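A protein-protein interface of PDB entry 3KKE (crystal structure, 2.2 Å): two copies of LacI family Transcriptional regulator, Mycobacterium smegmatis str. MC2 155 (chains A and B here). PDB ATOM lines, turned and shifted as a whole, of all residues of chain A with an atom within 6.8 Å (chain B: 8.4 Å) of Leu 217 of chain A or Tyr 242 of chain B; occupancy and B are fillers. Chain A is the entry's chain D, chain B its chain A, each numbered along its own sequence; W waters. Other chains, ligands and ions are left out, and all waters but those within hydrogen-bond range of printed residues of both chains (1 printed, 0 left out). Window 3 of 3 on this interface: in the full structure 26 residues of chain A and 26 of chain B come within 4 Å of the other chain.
O of Thr 240 of chain B sits at hydrogen-bond distance from OG of Ser 214 of chain A, 3.0 Å away. The guanidinium group (NH1) of Arg 218 of chain A is in salt-bridge range of the side-chain carboxylate (OE2) of Glu 288 of chain B.
The backbone NH (N) of Glu 288 of chain B is in hydrogen-bond range of the backbone carbonyl oxygen (O) of Ala 244 of chain B.
Among the printed residues, merely in contact across the chains: Ser 214 of chain A with Val 241 of chain B (3.7 Å), Leu 217 of chain A with Tyr 242 of chain B (3.8 Å), Arg 218 of chain A with Tyr 242 of chain B (3.6 Å), Arg 218 of chain A with Ala 244 of chain B (3.97 Å) and Tyr 242 of chain A with Leu 217 of chain B (3.8 Å).
Of chain B, only Tyr 242 comes within 4 Å of Leu 217 of chain A. Tyr 242 of chain B touches two residues of chain A. Of the printed residues of chain A, Ala 244 of chain B touches Arg 218 (3.97 Å). Of the printed residues of chain A, Leu 217 of chain B touches Tyr 242 (3.8 Å). Of the printed residues of chain A, Val 241 of chain B touches Ser 214. Of the printed residues of chain B, Ser 214 of chain A touches Thr 240 (3.0 Å) and Val 241 (3.7 Å). Asp 239 of chain B touches none of the printed residues of chain A. Thr 289 of chain B touches none of the printed residues of chain A. The nearest residue of chain B that does not touch Leu 217 of chain A is Pro 243 of chain B (6.8 Å). The nearest residue of chain A that does not touch Tyr 242 of chain B is Ser 214 of chain A (4.1 Å).
Of the 17 printed residues of chain B, 6 touch a printed residue of chain A. Printed residues of chain A that touch a printed residue of chain B: Ser 214, Leu 217, Arg 218 and Tyr 242.
Leu 217 of chain A touches Tyr 242 of chain B, and with the chains exchanged Tyr 242 of chain A touches Leu 217 of chain B.
Water W1 lies within hydrogen-bond range of the backbone carbonyl oxygen (O) of Tyr 242 of chain A and the backbone carbonyl oxygen (O) of Tyr 242 of chain B.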
ATOM      1  N   LEU A 183      -9.136  39.813  28.502  1.00  0.00           N
ATOM      2  CA  LEU A 183      -7.899  39.934  27.734  1.00  0.00           C
ATOM      3  C   LEU A 183      -7.986  41.122  26.783  1.00  0.00           C
ATOM      4  O   LEU A 183      -7.051  41.924  26.712  1.00  0.00           O
ATOM      5  CB  LEU A 183      -7.600  38.634  26.966  1.00  0.00           C
ATOM      6  CG  LEU A 183      -6.156  38.333  26.597  1.00  0.00           C
ATOM      7  CD1 LEU A 183      -5.699  39.282  25.510  1.00  0.00           C
ATOM      8  CD2 LEU A 183      -5.263  38.395  27.813  1.00  0.00           C
ATOM      9  N   ALA A 212      -8.488  33.411  27.093  1.00  0.00           N
ATOM     10  CA  ALA A 212      -7.467  34.480  26.973  1.00  0.00           C
ATOM     11  C   ALA A 212      -6.462  34.182  25.847  1.00  0.00           C
ATOM     12  O   ALA A 212      -6.164  35.022  25.003  1.00  0.00           O
ATOM     13  CB  ALA A 212      -6.749  34.679  28.304  1.00  0.00           C
ATOM     14  N   LEU A 213      -5.990  32.943  25.827  1.00  0.00           N
ATOM     15  CA  LEU A 213      -5.089  32.457  24.787  1.00  0.00           C
ATOM     16  C   LEU A 213      -5.654  32.712  23.402  1.00  0.00           C
ATOM     17  O   LEU A 213      -5.035  33.417  22.588  1.00  0.00           O
ATOM     18  CB  LEU A 213      -4.794  30.988  25.022  1.00  0.00           C
ATOM     19  CG  LEU A 213      -3.875  30.242  24.075  1.00  0.00           C
ATOM     20  CD1 LEU A 213      -2.540  30.970  23.955  1.00  0.00           C
ATOM     21  CD2 LEU A 213      -3.680  28.787  24.547  1.00  0.00           C
ATOM     22  N   SER A 214      -6.838  32.169  23.155  1.00  0.00           N
ATOM     23  CA  SER A 214      -7.492  32.284  21.858  1.00  0.00           C
ATOM     24  C   SER A 214      -7.567  33.724  21.391  1.00  0.00           C
ATOM     25  O   SER A 214      -7.269  34.010  20.236  1.00  0.00           O
ATOM     26  CB  SER A 214      -8.902  31.684  21.890  1.00  0.00           C
ATOM     27  OG  SER A 214      -8.852  30.341  22.323  1.00  0.00           O
ATOM     28  N   THR A 215      -7.968  34.613  22.284  1.00  0.00           N
ATOM     29  CA  THR A 215      -8.159  36.034  21.949  1.00  0.00           C
ATOM     30  C   THR A 215      -6.823  36.713  21.751  1.00  0.00           C
ATOM     31  O   THR A 215      -6.688  37.565  20.877  1.00  0.00           O
ATOM     32  CB  THR A 215      -8.942  36.784  23.038  1.00  0.00           C
ATOM     33  OG1 THR A 215     -10.328  36.496  22.896  1.00  0.00           O
ATOM     34  CG2 THR A 215      -8.747  38.319  22.924  1.00  0.00           C
ATOM     35  N   ALA A 216      -5.848  36.333  22.570  1.00  0.00           N
ATOM     36  CA  ALA A 216      -4.452  36.764  22.382  1.00  0.00           C
ATOM     37  C   ALA A 216      -3.968  36.488  20.961  1.00  0.00           C
ATOM     38  O   ALA A 216      -3.400  37.353  20.308  1.00  0.00           O
ATOM     39  CB  ALA A 216      -3.554  36.066  23.377  1.00  0.00           C
ATOM     40  N   LEU A 217      -4.229  35.277  20.481  1.00  0.00           N
ATOM     41  CA  LEU A 217      -3.735  34.844  19.174  1.00  0.00           C
ATOM     42  C   LEU A 217      -4.483  35.549  18.064  1.00  0.00           C
ATOM     43  O   LEU A 217      -3.876  36.007  17.091  1.00  0.00           O
ATOM     44  CB  LEU A 217      -3.875  33.326  19.035  1.00  0.00           C
ATOM     45  CG  LEU A 217      -2.835  32.531  19.815  1.00  0.00           C
ATOM     46  CD1 LEU A 217      -3.166  31.059  19.771  1.00  0.00           C
ATOM     47  CD2 LEU A 217      -1.437  32.780  19.222  1.00  0.00           C
ATOM     48  N   ARG A 218      -5.803  35.645  18.213  1.00  0.00           N
ATOM     49  CA  ARG A 218      -6.626  36.304  17.205  1.00  0.00           C
ATOM     50  C   ARG A 218      -6.145  37.721  16.940  1.00  0.00           C
ATOM     51  O   ARG A 218      -6.051  38.139  15.775  1.00  0.00           O
ATOM     52  CB  ARG A 218      -8.079  36.376  17.645  1.00  0.00           C
ATOM     53  CG  ARG A 218      -8.824  35.078  17.535  1.00  0.00           C
ATOM     54  CD  ARG A 218     -10.306  35.264  17.861  1.00  0.00           C
ATOM     55  NE  ARG A 218     -11.050  34.028  17.617  1.00  0.00           N
ATOM     56  CZ  ARG A 218     -11.307  33.541  16.407  1.00  0.00           C
ATOM     57  NH1 ARG A 218     -10.882  34.172  15.298  1.00  0.00           N
ATOM     58  NH2 ARG A 218     -11.988  32.403  16.304  1.00  0.00           N
ATOM     59  N   LEU A 219      -5.869  38.441  18.031  1.00  0.00           N
ATOM     60  CA  LEU A 219      -5.446  39.843  17.978  1.00  0.00           C
ATOM     61  C   LEU A 219      -4.156  39.981  17.143  1.00  0.00           C
ATOM     62  O   LEU A 219      -3.990  40.939  16.403  1.00  0.00           O
ATOM     63  CB  LEU A 219      -5.264  40.419  19.404  1.00  0.00           C
ATOM     64  CG  LEU A 219      -6.526  40.773  20.219  1.00  0.00           C
ATOM     65  CD1 LEU A 219      -6.231  40.963  21.717  1.00  0.00           C
ATOM     66  CD2 LEU A 219      -7.210  42.014  19.665  1.00  0.00           C
ATOM     67  N   GLY A 220      -3.275  38.994  17.253  1.00  0.00           N
ATOM     68  CA  GLY A 220      -1.992  39.008  16.578  1.00  0.00           C
ATOM     69  C   GLY A 220      -0.832  39.092  17.547  1.00  0.00           C
ATOM     70  O   GLY A 220       0.289  39.400  17.136  1.00  0.00           O
ATOM     71  N   LEU A 221      -1.093  38.844  18.836  1.00  0.00           N
ATOM     72  CA  LEU A 221      -0.016  38.634  19.797  1.00  0.00           C
ATOM     73  C   LEU A 221       0.510  37.202  19.670  1.00  0.00           C
ATOM     74  O   LEU A 221      -0.276  36.237  19.721  1.00  0.00           O
ATOM     75  CB  LEU A 221      -0.505  38.836  21.228  1.00  0.00           C
ATOM     76  CG  LEU A 221      -1.019  40.198  21.700  1.00  0.00           C
ATOM     77  CD1 LEU A 221      -1.505  40.084  23.149  1.00  0.00           C
ATOM     78  CD2 LEU A 221       0.067  41.269  21.572  1.00  0.00           C
ATOM     79  N   ARG A 222       1.821  37.047  19.496  1.00  0.00           N
ATOM     80  CA  ARG A 222       2.433  35.718  19.583  1.00  0.00           C
ATOM     81  C   ARG A 222       2.498  35.318  21.067  1.00  0.00           C
ATOM     82  O   ARG A 222       2.785  36.151  21.919  1.00  0.00           O
ATOM     83  CB  ARG A 222       3.824  35.678  18.921  1.00  0.00           C
ATOM     84  N   VAL A 223       2.163  34.061  21.367  1.00  0.00           N
ATOM     85  CA  VAL A 223       2.309  33.514  22.704  1.00  0.00           C
ATOM     86  C   VAL A 223       3.252  32.330  22.584  1.00  0.00           C
ATOM     87  O   VAL A 223       3.010  31.454  21.754  1.00  0.00           O
ATOM     88  CB  VAL A 223       0.931  33.067  23.257  1.00  0.00           C
ATOM     89  CG1 VAL A 223       1.064  32.343  24.603  1.00  0.00           C
ATOM     90  CG2 VAL A 223      -0.016  34.268  23.380  1.00  0.00           C
ATOM     91  N   ILE A 229       1.130  33.349  29.271  1.00  0.00           N
ATOM     92  CA  ILE A 229      -0.143  33.029  29.946  1.00  0.00           C
ATOM     93  C   ILE A 229      -0.013  31.796  30.851  1.00  0.00           C
ATOM     94  O   ILE A 229       0.424  30.729  30.403  1.00  0.00           O
ATOM     95  CB  ILE A 229      -1.309  32.802  28.915  1.00  0.00           C
ATOM     96  CG1 ILE A 229      -1.320  33.880  27.820  1.00  0.00           C
ATOM     97  CG2 ILE A 229      -2.665  32.821  29.598  1.00  0.00           C
ATOM     98  CD1 ILE A 229      -2.384  33.676  26.703  1.00  0.00           C
ATOM     99  N   TYR A 242      -3.003  24.082  21.204  1.00  0.00           N
ATOM    100  CA  TYR A 242      -1.679  24.496  20.724  1.00  0.00           C
ATOM    101  C   TYR A 242      -1.631  25.994  20.479  1.00  0.00           C
ATOM    102  O   TYR A 242      -2.399  26.515  19.666  1.00  0.00           O
ATOM    103  CB  TYR A 242      -1.310  23.801  19.437  1.00  0.00           C
ATOM    104  CG  TYR A 242       0.084  24.123  18.965  1.00  0.00           C
ATOM    105  CD1 TYR A 242       1.175  23.534  19.565  1.00  0.00           C
ATOM    106  CD2 TYR A 242       0.310  25.027  17.917  1.00  0.00           C
ATOM    107  CE1 TYR A 242       2.453  23.817  19.154  1.00  0.00           C
ATOM    108  CE2 TYR A 242       1.599  25.316  17.488  1.00  0.00           C
ATOM    109  CZ  TYR A 242       2.667  24.694  18.114  1.00  0.00           C
ATOM    110  OH  TYR A 242       3.966  24.921  17.731  1.00  0.00           O
ATOM    111  N   PRO A 243      -0.735  26.697  21.187  1.00  0.00           N
ATOM    112  CA  PRO A 243       0.166  26.163  22.224  1.00  0.00           C
ATOM    113  C   PRO A 243      -0.558  25.696  23.485  1.00  0.00           C
ATOM    114  O   PRO A 243      -1.556  26.284  23.873  1.00  0.00           O
ATOM    115  CB  PRO A 243       1.067  27.372  22.559  1.00  0.00           C
ATOM    116  CG  PRO A 243       0.196  28.540  22.306  1.00  0.00           C
ATOM    117  CD  PRO A 243      -0.599  28.160  21.059  1.00  0.00           C
ATOM    118  N   VAL B 210     -10.678  18.204  18.329  1.00  0.00           N
ATOM    119  CA  VAL B 210      -9.820  19.200  18.976  1.00  0.00           C
ATOM    120  C   VAL B 210      -8.410  18.665  19.131  1.00  0.00           C
ATOM    121  O   VAL B 210      -7.440  19.368  18.843  1.00  0.00           O
ATOM    122  CB  VAL B 210     -10.391  19.616  20.346  1.00  0.00           C
ATOM    123  CG1 VAL B 210      -9.396  20.567  21.088  1.00  0.00           C
ATOM    124  CG2 VAL B 210     -11.752  20.278  20.153  1.00  0.00           C
ATOM    125  N   LEU B 213      -6.888  18.731  15.592  1.00  0.00           N
ATOM    126  CA  LEU B 213      -6.523  20.061  15.156  1.00  0.00           C
ATOM    127  C   LEU B 213      -5.201  20.426  15.821  1.00  0.00           C
ATOM    128  O   LEU B 213      -4.262  20.895  15.162  1.00  0.00           O
ATOM    129  CB  LEU B 213      -7.631  21.072  15.486  1.00  0.00           C
ATOM    130  CG  LEU B 213      -7.309  22.582  15.426  1.00  0.00           C
ATOM    131  CD1 LEU B 213      -6.995  22.983  14.026  1.00  0.00           C
ATOM    132  CD2 LEU B 213      -8.453  23.452  15.963  1.00  0.00           C
ATOM    133  N   SER B 214      -5.102  20.179  17.118  1.00  0.00           N
ATOM    134  CA  SER B 214      -3.876  20.464  17.819  1.00  0.00           C
ATOM    135  C   SER B 214      -2.675  19.753  17.230  1.00  0.00           C
ATOM    136  O   SER B 214      -1.622  20.341  17.069  1.00  0.00           O
ATOM    137  CB  SER B 214      -3.986  20.080  19.294  1.00  0.00           C
ATOM    138  OG  SER B 214      -5.108  20.715  19.886  1.00  0.00           O
ATOM    139  N   LEU B 217      -1.592  21.170  13.976  1.00  0.00           N
ATOM    140  CA  LEU B 217      -0.833  22.394  14.195  1.00  0.00           C
ATOM    141  C   LEU B 217       0.594  22.090  14.703  1.00  0.00           C
ATOM    142  O   LEU B 217       1.554  22.633  14.167  1.00  0.00           O
ATOM    143  CB  LEU B 217      -1.584  23.356  15.121  1.00  0.00           C
ATOM    144  CG  LEU B 217      -2.888  23.920  14.534  1.00  0.00           C
ATOM    145  CD1 LEU B 217      -3.688  24.655  15.592  1.00  0.00           C
ATOM    146  CD2 LEU B 217      -2.638  24.807  13.290  1.00  0.00           C
ATOM    147  N   VAL B 223      -3.758  25.001   9.097  1.00  0.00           N
ATOM    148  CA  VAL B 223      -5.192  24.735   9.067  1.00  0.00           C
ATOM    149  C   VAL B 223      -5.908  26.063   8.944  1.00  0.00           C
ATOM    150  O   VAL B 223      -5.807  26.902   9.839  1.00  0.00           O
ATOM    151  CB  VAL B 223      -5.686  24.035  10.363  1.00  0.00           C
ATOM    152  CG1 VAL B 223      -7.150  23.845  10.307  1.00  0.00           C
ATOM    153  CG2 VAL B 223      -5.017  22.714  10.561  1.00  0.00           C
ATOM    154  N   PRO B 224      -6.692  26.259   7.880  1.00  0.00           N
ATOM    155  CA  PRO B 224      -7.179  25.321   6.873  1.00  0.00           C
ATOM    156  C   PRO B 224      -6.342  25.116   5.570  1.00  0.00           C
ATOM    157  O   PRO B 224      -6.704  24.255   4.746  1.00  0.00           O
ATOM    158  CB  PRO B 224      -8.543  25.894   6.532  1.00  0.00           C
ATOM    159  CG  PRO B 224      -8.334  27.389   6.652  1.00  0.00           C
ATOM    160  CD  PRO B 224      -7.373  27.569   7.789  1.00  0.00           C
ATOM    161  N   VAL B 237     -15.481  24.581  23.636  1.00  0.00           N
ATOM    162  CA  VAL B 237     -14.099  24.349  23.233  1.00  0.00           C
ATOM    163  C   VAL B 237     -13.922  24.458  21.725  1.00  0.00           C
ATOM    164  O   VAL B 237     -12.971  25.082  21.248  1.00  0.00           O
ATOM    165  CB  VAL B 237     -13.635  22.948  23.661  1.00  0.00           C
ATOM    166  CG1 VAL B 237     -12.185  22.699  23.250  1.00  0.00           C
ATOM    167  CG2 VAL B 237     -13.874  22.722  25.202  1.00  0.00           C
ATOM    168  N   SER B 238     -14.829  23.847  20.960  1.00  0.00           N
ATOM    169  CA  SER B 238     -14.653  23.842  19.501  1.00  0.00           C
ATOM    170  C   SER B 238     -14.874  25.232  18.988  1.00  0.00           C
ATOM    171  O   SER B 238     -14.326  25.598  17.955  1.00  0.00           O
ATOM    172  CB  SER B 238     -15.581  22.853  18.788  1.00  0.00           C
ATOM    173  OG  SER B 238     -16.941  23.199  18.914  1.00  0.00           O
ATOM    174  N   ASP B 239     -15.691  25.991  19.717  1.00  0.00           N
ATOM    175  CA  ASP B 239     -16.017  27.353  19.330  1.00  0.00           C
ATOM    176  C   ASP B 239     -15.022  28.408  19.863  1.00  0.00           C
ATOM    177  O   ASP B 239     -15.033  29.544  19.410  1.00  0.00           O
ATOM    178  CB  ASP B 239     -17.407  27.706  19.803  1.00  0.00           C
ATOM    179  CG  ASP B 239     -18.458  27.482  18.763  1.00  0.00           C
ATOM    180  OD1 ASP B 239     -18.159  27.248  17.561  1.00  0.00           O
ATOM    181  OD2 ASP B 239     -19.637  27.578  19.160  1.00  0.00           O
ATOM    182  N   THR B 240     -14.172  28.021  20.804  1.00  0.00           N
ATOM    183  CA  THR B 240     -13.285  28.946  21.457  1.00  0.00           C
ATOM    184  C   THR B 240     -11.893  28.905  20.884  1.00  0.00           C
ATOM    185  O   THR B 240     -11.311  29.951  20.621  1.00  0.00           O
ATOM    186  CB  THR B 240     -13.203  28.684  22.948  1.00  0.00           C
ATOM    187  OG1 THR B 240     -14.504  28.813  23.494  1.00  0.00           O
ATOM    188  CG2 THR B 240     -12.276  29.714  23.615  1.00  0.00           C
ATOM    189  N   VAL B 241     -11.372  27.708  20.676  1.00  0.00           N
ATOM    190  CA  VAL B 241      -9.998  27.548  20.235  1.00  0.00           C
ATOM    191  C   VAL B 241      -9.744  28.297  18.942  1.00  0.00           C
ATOM    192  O   VAL B 241     -10.674  28.709  18.233  1.00  0.00           O
ATOM    193  CB  VAL B 241      -9.611  26.057  20.093  1.00  0.00           C
ATOM    194  CG1 VAL B 241      -9.777  25.345  21.435  1.00  0.00           C
ATOM    195  CG2 VAL B 241     -10.435  25.348  18.989  1.00  0.00           C
ATOM    196  N   TYR B 242      -8.465  28.510  18.654  1.00  0.00           N
ATOM    197  CA  TYR B 242      -8.064  29.268  17.489  1.00  0.00           C
ATOM    198  C   TYR B 242      -7.113  28.446  16.657  1.00  0.00           C
ATOM    199  O   TYR B 242      -6.056  28.052  17.167  1.00  0.00           O
ATOM    200  CB  TYR B 242      -7.353  30.565  17.897  1.00  0.00           C
ATOM    201  CG  TYR B 242      -6.958  31.371  16.701  1.00  0.00           C
ATOM    202  CD1 TYR B 242      -7.921  32.033  15.949  1.00  0.00           C
ATOM    203  CD2 TYR B 242      -5.634  31.444  16.296  1.00  0.00           C
ATOM    204  CE1 TYR B 242      -7.573  32.761  14.819  1.00  0.00           C
ATOM    205  CE2 TYR B 242      -5.266  32.191  15.165  1.00  0.00           C
ATOM    206  CZ  TYR B 242      -6.245  32.844  14.436  1.00  0.00           C
ATOM    207  OH  TYR B 242      -5.913  33.572  13.309  1.00  0.00           O
ATOM    208  N   PRO B 243      -7.467  28.174  15.386  1.00  0.00           N
ATOM    209  CA  PRO B 243      -8.706  28.544  14.691  1.00  0.00           C
ATOM    210  C   PRO B 243      -9.901  27.726  15.240  1.00  0.00           C
ATOM    211  O   PRO B 243      -9.699  26.645  15.777  1.00  0.00           O
ATOM    212  CB  PRO B 243      -8.409  28.162  13.232  1.00  0.00           C
ATOM    213  CG  PRO B 243      -7.520  26.991  13.346  1.00  0.00           C
ATOM    214  CD  PRO B 243      -6.647  27.265  14.574  1.00  0.00           C
ATOM    215  N   ALA B 244     -11.101  28.282  15.153  1.00  0.00           N
ATOM    216  CA  ALA B 244     -12.294  27.671  15.715  1.00  0.00           C
ATOM    217  C   ALA B 244     -12.747  26.548  14.776  1.00  0.00           C
ATOM    218  O   ALA B 244     -12.821  26.741  13.561  1.00  0.00           O
ATOM    219  CB  ALA B 244     -13.396  28.714  15.895  1.00  0.00           C
ATOM    220  N   LEU B 245     -13.020  25.380  15.350  1.00  0.00           N
ATOM    221  CA  LEU B 245     -13.388  24.182  14.579  1.00  0.00           C
ATOM    222  C   LEU B 245     -14.731  24.307  13.948  1.00  0.00           C
ATOM    223  O   LEU B 245     -15.706  24.560  14.638  1.00  0.00           O
ATOM    224  CB  LEU B 245     -13.461  22.965  15.478  1.00  0.00           C
ATOM    225  CG  LEU B 245     -12.216  22.106  15.506  1.00  0.00           C
ATOM    226  CD1 LEU B 245     -12.258  21.156  16.705  1.00  0.00           C
ATOM    227  CD2 LEU B 245     -12.131  21.362  14.181  1.00  0.00           C
ATOM    228  N   GLU B 288     -13.530  28.207  11.207  1.00  0.00           N
ATOM    229  CA  GLU B 288     -12.249  28.614  10.594  1.00  0.00           C
ATOM    230  C   GLU B 288     -11.335  27.479  10.144  1.00  0.00           C
ATOM    231  O   GLU B 288     -10.206  27.735   9.710  1.00  0.00           O
ATOM    232  CB  GLU B 288     -11.484  29.533  11.566  1.00  0.00           C
ATOM    233  CG  GLU B 288     -12.196  30.846  11.818  1.00  0.00           C
ATOM    234  CD  GLU B 288     -11.862  31.491  13.160  1.00  0.00           C
ATOM    235  OE1 GLU B 288     -11.132  30.922  13.981  1.00  0.00           O
ATOM    236  OE2 GLU B 288     -12.342  32.607  13.390  1.00  0.00           O
ATOM    237  N   THR B 289     -11.807  26.227  10.217  1.00  0.00           N
ATOM    238  CA  THR B 289     -10.937  25.107   9.930  1.00  0.00           C
ATOM    239  C   THR B 289     -11.262  24.424   8.624  1.00  0.00           C
ATOM    240  O   THR B 289     -10.751  23.351   8.361  1.00  0.00           O
ATOM    241  CB  THR B 289     -10.930  24.063  11.066  1.00  0.00           C
ATOM    242  OG1 THR B 289     -12.264  23.633  11.324  1.00  0.00           O
ATOM    243  CG2 THR B 289     -10.270  24.650  12.316  1.00  0.00           C
HETATM  244  O   HOH W   1      -2.729  28.260  16.849  1.00  0.00           O
